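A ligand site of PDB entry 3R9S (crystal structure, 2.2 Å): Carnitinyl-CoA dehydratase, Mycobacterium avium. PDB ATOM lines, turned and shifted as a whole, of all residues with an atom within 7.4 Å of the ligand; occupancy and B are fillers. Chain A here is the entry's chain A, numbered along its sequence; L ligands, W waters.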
ATOM      1  N   GLY A  70      -6.612  28.727 -33.940  1.00  0.00           N
ATOM      2  CA  GLY A  70      -6.468  27.743 -32.875  1.00  0.00           C
ATOM      3  C   GLY A  70      -7.400  28.037 -31.723  1.00  0.00           C
ATOM      4  O   GLY A  70      -8.316  28.838 -31.840  1.00  0.00           O
ATOM      5  N   ALA A  71      -7.170  27.362 -30.614  1.00  0.00           N
ATOM      6  CA  ALA A  71      -7.938  27.589 -29.403  1.00  0.00           C
ATOM      7  C   ALA A  71      -7.540  28.968 -28.902  1.00  0.00           C
ATOM      8  O   ALA A  71      -6.381  29.372 -29.058  1.00  0.00           O
ATOM      9  CB  ALA A  71      -7.599  26.528 -28.373  1.00  0.00           C
ATOM     10  N   ASP A  72      -8.500  29.704 -28.343  1.00  0.00           N
ATOM     11  CA  ASP A  72      -8.218  31.063 -27.856  1.00  0.00           C
ATOM     12  C   ASP A  72      -7.343  30.990 -26.607  1.00  0.00           C
ATOM     13  O   ASP A  72      -7.779  30.555 -25.545  1.00  0.00           O
ATOM     14  CB  ASP A  72      -9.496  31.854 -27.596  1.00  0.00           C
ATOM     15  CG  ASP A  72      -9.216  33.330 -27.294  1.00  0.00           C
ATOM     16  OD1 ASP A  72      -8.568  33.628 -26.266  1.00  0.00           O
ATOM     17  OD2 ASP A  72      -9.667  34.196 -28.092  1.00  0.00           O
ATOM     18  N   LEU A  73      -6.097  31.421 -26.753  1.00  0.00           N
ATOM     19  CA  LEU A  73      -5.110  31.263 -25.700  1.00  0.00           C
ATOM     20  C   LEU A  73      -5.360  32.222 -24.521  1.00  0.00           C
ATOM     21  O   LEU A  73      -5.020  31.915 -23.391  1.00  0.00           O
ATOM     22  CB  LEU A  73      -3.702  31.438 -26.275  1.00  0.00           C
ATOM     23  CG  LEU A  73      -3.326  30.434 -27.385  1.00  0.00           C
ATOM     24  CD1 LEU A  73      -2.002  30.825 -28.083  1.00  0.00           C
ATOM     25  CD2 LEU A  73      -3.234  29.025 -26.845  1.00  0.00           C
ATOM     26  N   ILE A  76      -7.861  30.400 -22.456  1.00  0.00           N
ATOM     27  CA  ILE A  76      -7.194  29.351 -21.700  1.00  0.00           C
ATOM     28  C   ILE A  76      -6.490  29.919 -20.466  1.00  0.00           C
ATOM     29  O   ILE A  76      -6.593  29.367 -19.377  1.00  0.00           O
ATOM     30  CB  ILE A  76      -6.175  28.573 -22.528  1.00  0.00           C
ATOM     31  CG1 ILE A  76      -6.886  27.758 -23.613  1.00  0.00           C
ATOM     32  CG2 ILE A  76      -5.361  27.644 -21.617  1.00  0.00           C
ATOM     33  CD1 ILE A  76      -5.965  27.194 -24.694  1.00  0.00           C
ATOM     34  N   LEU A  82     -13.889  26.590 -23.328  1.00  0.00           N
ATOM     35  CA  LEU A  82     -13.943  26.954 -24.747  1.00  0.00           C
ATOM     36  C   LEU A  82     -15.130  26.369 -25.484  1.00  0.00           C
ATOM     37  O   LEU A  82     -15.431  26.777 -26.608  1.00  0.00           O
ATOM     38  CB  LEU A  82     -12.667  26.517 -25.461  1.00  0.00           C
ATOM     39  CG  LEU A  82     -11.335  27.024 -24.916  1.00  0.00           C
ATOM     40  CD1 LEU A  82     -10.226  26.479 -25.767  1.00  0.00           C
ATOM     41  CD2 LEU A  82     -11.275  28.522 -24.857  1.00  0.00           C
ATOM     42  N   PHE A  92     -14.518  20.596 -29.009  1.00  0.00           N
ATOM     43  CA  PHE A  92     -14.007  21.863 -29.502  1.00  0.00           C
ATOM     44  C   PHE A  92     -14.877  22.473 -30.608  1.00  0.00           C
ATOM     45  O   PHE A  92     -15.157  21.813 -31.613  1.00  0.00           O
ATOM     46  CB  PHE A  92     -12.590  21.599 -30.016  1.00  0.00           C
ATOM     47  CG  PHE A  92     -11.856  22.808 -30.491  1.00  0.00           C
ATOM     48  CD1 PHE A  92     -11.242  23.679 -29.592  1.00  0.00           C
ATOM     49  CD2 PHE A  92     -11.696  23.044 -31.847  1.00  0.00           C
ATOM     50  CE1 PHE A  92     -10.543  24.781 -30.037  1.00  0.00           C
ATOM     51  CE2 PHE A  92     -10.980  24.128 -32.289  1.00  0.00           C
ATOM     52  CZ  PHE A  92     -10.409  25.009 -31.367  1.00  0.00           C
ATOM     53  N   LEU A 113      -4.388  26.756 -38.004  1.00  0.00           N
ATOM     54  CA  LEU A 113      -3.375  26.124 -37.149  1.00  0.00           C
ATOM     55  C   LEU A 113      -3.988  25.580 -35.854  1.00  0.00           C
ATOM     56  O   LEU A 113      -4.906  26.179 -35.268  1.00  0.00           O
ATOM     57  CB  LEU A 113      -2.259  27.115 -36.815  1.00  0.00           C
ATOM     58  CG  LEU A 113      -1.343  27.531 -37.951  1.00  0.00           C
ATOM     59  CD1 LEU A 113      -0.418  28.672 -37.513  1.00  0.00           C
ATOM     60  CD2 LEU A 113      -0.556  26.339 -38.506  1.00  0.00           C
ATOM     61  N   GLY A 114      -3.469  24.436 -35.425  1.00  0.00           N
ATOM     62  CA  GLY A 114      -3.883  23.813 -34.193  1.00  0.00           C
ATOM     63  C   GLY A 114      -5.329  23.394 -34.294  1.00  0.00           C
ATOM     64  O   GLY A 114      -5.686  22.629 -35.195  1.00  0.00           O
ATOM     65  N   GLY A 115      -6.158  23.934 -33.400  1.00  0.00           N
ATOM     66  CA  GLY A 115      -7.610  23.769 -33.466  1.00  0.00           C
ATOM     67  C   GLY A 115      -8.201  23.982 -34.859  1.00  0.00           C
ATOM     68  O   GLY A 115      -9.109  23.264 -35.268  1.00  0.00           O
ATOM     69  N   GLY A 116      -7.653  24.953 -35.594  1.00  0.00           N
ATOM     70  CA  GLY A 116      -8.057  25.187 -36.964  1.00  0.00           C
ATOM     71  C   GLY A 116      -7.819  23.985 -37.880  1.00  0.00           C
ATOM     72  O   GLY A 116      -8.674  23.627 -38.681  1.00  0.00           O
ATOM     73  N   GLU A 118      -7.620  21.029 -36.740  1.00  0.00           N
ATOM     74  CA  GLU A 118      -8.495  20.010 -36.165  1.00  0.00           C
ATOM     75  C   GLU A 118      -9.951  20.130 -36.625  1.00  0.00           C
ATOM     76  O   GLU A 118     -10.634  19.130 -36.748  1.00  0.00           O
ATOM     77  CB  GLU A 118      -8.394  20.016 -34.632  1.00  0.00           C
ATOM     78  CG  GLU A 118      -7.072  19.455 -34.128  1.00  0.00           C
ATOM     79  CD  GLU A 118      -6.894  19.624 -32.630  1.00  0.00           C
ATOM     80  OE1 GLU A 118      -6.843  20.783 -32.161  1.00  0.00           O
ATOM     81  OE2 GLU A 118      -6.804  18.589 -31.919  1.00  0.00           O
ATOM     82  N   LEU A 136      -0.134  21.511 -36.498  1.00  0.00           N
ATOM     83  CA  LEU A 136      -0.506  21.260 -35.111  1.00  0.00           C
ATOM     84  C   LEU A 136       0.633  21.680 -34.192  1.00  0.00           C
ATOM     85  O   LEU A 136       1.349  20.831 -33.655  1.00  0.00           O
ATOM     86  CB  LEU A 136      -0.837  19.782 -34.891  1.00  0.00           C
ATOM     87  CG  LEU A 136      -2.080  19.237 -35.609  1.00  0.00           C
ATOM     88  CD1 LEU A 136      -2.149  17.706 -35.425  1.00  0.00           C
ATOM     89  CD2 LEU A 136      -3.332  19.900 -35.125  1.00  0.00           C
ATOM     90  N   PRO A 137       0.793  23.004 -33.982  1.00  0.00           N
ATOM     91  CA  PRO A 137       1.907  23.554 -33.216  1.00  0.00           C
ATOM     92  C   PRO A 137       1.704  23.519 -31.705  1.00  0.00           C
ATOM     93  O   PRO A 137       2.477  24.151 -30.958  1.00  0.00           O
ATOM     94  CB  PRO A 137       1.951  25.017 -33.692  1.00  0.00           C
ATOM     95  CG  PRO A 137       0.540  25.358 -33.938  1.00  0.00           C
ATOM     96  CD  PRO A 137      -0.102  24.078 -34.468  1.00  0.00           C
ATOM     97  N   GLU A 138       0.662  22.818 -31.254  1.00  0.00           N
ATOM     98  CA  GLU A 138       0.318  22.779 -29.846  1.00  0.00           C
ATOM     99  C   GLU A 138       1.535  22.395 -28.994  1.00  0.00           C
ATOM    100  O   GLU A 138       1.759  23.003 -27.958  1.00  0.00           O
ATOM    101  CB  GLU A 138      -0.862  21.819 -29.591  1.00  0.00           C
ATOM    102  CG  GLU A 138      -2.242  22.357 -30.008  1.00  0.00           C
ATOM    103  CD  GLU A 138      -2.643  21.997 -31.430  1.00  0.00           C
ATOM    104  OE1 GLU A 138      -1.746  21.741 -32.267  1.00  0.00           O
ATOM    105  OE2 GLU A 138      -3.869  21.946 -31.710  1.00  0.00           O
ATOM    106  N   LEU A 143       1.003  22.479 -25.054  1.00  0.00           N
ATOM    107  CA  LEU A 143      -0.359  21.940 -25.195  1.00  0.00           C
ATOM    108  C   LEU A 143      -0.273  20.677 -26.063  1.00  0.00           C
ATOM    109  O   LEU A 143       0.796  20.374 -26.568  1.00  0.00           O
ATOM    110  CB  LEU A 143      -1.277  22.977 -25.861  1.00  0.00           C
ATOM    111  CG  LEU A 143      -1.458  24.334 -25.146  1.00  0.00           C
ATOM    112  CD1 LEU A 143      -2.282  25.303 -25.996  1.00  0.00           C
ATOM    113  CD2 LEU A 143      -2.063  24.160 -23.749  1.00  0.00           C
ATOM    114  N   ILE A 144      -1.375  19.949 -26.196  1.00  0.00           N
ATOM    115  CA  ILE A 144      -1.515  18.942 -27.220  1.00  0.00           C
ATOM    116  C   ILE A 144      -2.741  19.212 -28.096  1.00  0.00           C
ATOM    117  O   ILE A 144      -3.592  20.035 -27.757  1.00  0.00           O
ATOM    118  CB  ILE A 144      -1.554  17.510 -26.660  1.00  0.00           C
ATOM    119  CG1 ILE A 144      -2.748  17.339 -25.694  1.00  0.00           C
ATOM    120  CG2 ILE A 144      -0.208  17.145 -25.971  1.00  0.00           C
ATOM    121  CD1 ILE A 144      -3.095  15.903 -25.371  1.00  0.00           C
ATOM    122  N   ALA A 145      -2.824  18.515 -29.238  1.00  0.00           N
ATOM    123  CA  ALA A 145      -3.954  18.620 -30.150  1.00  0.00           C
ATOM    124  C   ALA A 145      -5.066  17.750 -29.584  1.00  0.00           C
ATOM    125  O   ALA A 145      -5.335  16.634 -30.055  1.00  0.00           O
ATOM    126  CB  ALA A 145      -3.570  18.182 -31.561  1.00  0.00           C
ATOM    127  N   ALA A 146      -5.709  18.278 -28.559  1.00  0.00           N
ATOM    128  CA  ALA A 146      -6.719  17.596 -27.791  1.00  0.00           C
ATOM    129  C   ALA A 146      -8.094  17.562 -28.462  1.00  0.00           C
ATOM    130  O   ALA A 146      -8.973  16.866 -27.997  1.00  0.00           O
ATOM    131  CB  ALA A 146      -6.848  18.270 -26.403  1.00  0.00           C
ATOM    132  N   ALA A 147      -8.297  18.380 -29.489  1.00  0.00           N
ATOM    133  CA  ALA A 147      -9.558  18.423 -30.207  1.00  0.00           C
ATOM    134  C   ALA A 147      -9.552  17.426 -31.385  1.00  0.00           C
ATOM    135  O   ALA A 147     -10.038  17.757 -32.471  1.00  0.00           O
ATOM    136  CB  ALA A 147      -9.846  19.865 -30.695  1.00  0.00           C
ATOM    137  N   GLY A 148      -8.994  16.238 -31.163  1.00  0.00           N
ATOM    138  CA  GLY A 148      -8.978  15.130 -32.119  1.00  0.00           C
ATOM    139  C   GLY A 148      -7.692  14.999 -32.914  1.00  0.00           C
ATOM    140  O   GLY A 148      -7.423  13.940 -33.470  1.00  0.00           O
ATOM    141  N   GLY A 149      -6.916  16.068 -32.991  1.00  0.00           N
ATOM    142  CA  GLY A 149      -5.710  16.096 -33.804  1.00  0.00           C
ATOM    143  C   GLY A 149      -4.784  14.923 -33.537  1.00  0.00           C
ATOM    144  O   GLY A 149      -4.303  14.307 -34.484  1.00  0.00           O
ATOM    145  N   VAL A 150      -4.568  14.609 -32.257  1.00  0.00           N
ATOM    146  CA  VAL A 150      -3.575  13.599 -31.876  1.00  0.00           C
ATOM    147  C   VAL A 150      -3.873  12.207 -32.371  1.00  0.00           C
ATOM    148  O   VAL A 150      -2.942  11.458 -32.590  1.00  0.00           O
ATOM    149  CB  VAL A 150      -3.323  13.495 -30.326  1.00  0.00           C
ATOM    150  CG1 VAL A 150      -2.391  14.577 -29.870  1.00  0.00           C
ATOM    151  CG2 VAL A 150      -4.633  13.516 -29.513  1.00  0.00           C
ATOM    152  N   MET A 240      -4.409  14.425 -20.807  1.00  0.00           N
ATOM    153  CA  MET A 240      -4.618  15.848 -20.470  1.00  0.00           C
ATOM    154  C   MET A 240      -4.529  16.086 -18.967  1.00  0.00           C
ATOM    155  O   MET A 240      -3.947  17.065 -18.506  1.00  0.00           O
ATOM    156  CB  MET A 240      -5.994  16.289 -20.975  1.00  0.00           C
ATOM    157  CG  MET A 240      -5.995  17.556 -21.781  1.00  0.00           C
ATOM    158  SD  MET A 240      -7.209  17.498 -23.143  1.00  0.00           S
ATOM    159  CE  MET A 240      -8.677  16.842 -22.370  1.00  0.00           C
HETATM  160  C1  LIG L   1      -6.176  22.031 -29.228  1.00  0.00           C
HETATM  161  O1  LIG L   1      -5.266  22.646 -29.812  1.00  0.00           O
HETATM  162  O2  LIG L   1      -6.679  21.005 -29.733  1.00  0.00           O
HETATM  163  C2  LIG L   1      -6.672  22.553 -27.927  1.00  0.00           C
HETATM  164  C3  LIG L   1      -5.879  23.427 -27.206  1.00  0.00           C
HETATM  165  C4  LIG L   1      -6.334  23.945 -25.993  1.00  0.00           C
HETATM  166  C5  LIG L   1      -7.591  23.584 -25.510  1.00  0.00           C
HETATM  167  C6  LIG L   1      -8.388  22.690 -26.237  1.00  0.00           C
HETATM  168  C7  LIG L   1      -7.930  22.186 -27.451  1.00  0.00           C
HETATM  169  O   HOH W   1      -5.078  25.282 -30.856  1.00  0.00           O
HETATM  170  O   HOH W   2     -10.756  20.369 -26.619  1.00  0.00           O
HETATM  171  O   HOH W   3      -9.185  24.146 -22.593  1.00  0.00           O
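The backbone NH (N) of Ala 146 is in hydrogen-bond range of an oxygen (O2) of the ligand, 3.1 Å away. The side-chain carboxylate (OE1) of Glu 118 sits close to an oxygen (O2) of the ligand. N of Ala 147 is in hydrogen-bond range of O2 of the ligand (3.1 Å). An oxygen (O1) of the ligand lies close to the side-chain carboxylate (OE2) of Glu 138 (2.5 Å).
The backbone NH (N) of Gly 115 lies within hydrogen-bond range of the side-chain carboxylate (OE2) of Glu 138 (3.5 Å). The side-chain carboxylate of Glu 118 is in hydrogen-bond range of the backbone NH of Ala 147 (2.9 Å). N of Val 150 sits at hydrogen-bond distance from O of Ala 145, 3.1 Å away. The backbone carbonyl oxygen of Glu 138 is in hydrogen-bond range of the backbone NH of Leu 143. The backbone NH (N) of Gly 115 lies close to the side-chain carboxylate (OE1) of Glu 118 (3.5 Å). OE2 of Glu 118 is in hydrogen-bond range of N of Gly 149 (2.7 Å). The backbone NH (N) of Gly 148 lies within hydrogen-bond range of the side-chain carboxylate (OE2) of Glu 118 (3.3 Å).
Ala 71 touches the ligand. CD1 of Ile 76 touches C4 of the ligand, at 3.5 Å. Leu 82 touches the ligand (CD1 to C5, 3.9 Å). N of Gly 115 touches O1 of the ligand, at 3.9 Å. Ile 144 touches the ligand. Ala 145 touches the ligand (C to O2, 3.6 Å). Hydrophobic or aromatic side chains that line the ligand: Ala 71, Ile 76, Leu 82 and Ala 147. Within 4 Å of the ligand: Ala 71, Ile 76, Leu 82, Gly 115, Glu 118, Glu 138, Ile 144, Ala 145, Ala 146 and Ala 147. The nearest printed residue that does not touch the ligand is Phe 92 (4.2 Å).
Water W1 lies within hydrogen-bond range of O1 of the ligand (2.8 Å), N of Ala 71 (3.0 Å) and N of Gly 115 (3.1 Å).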
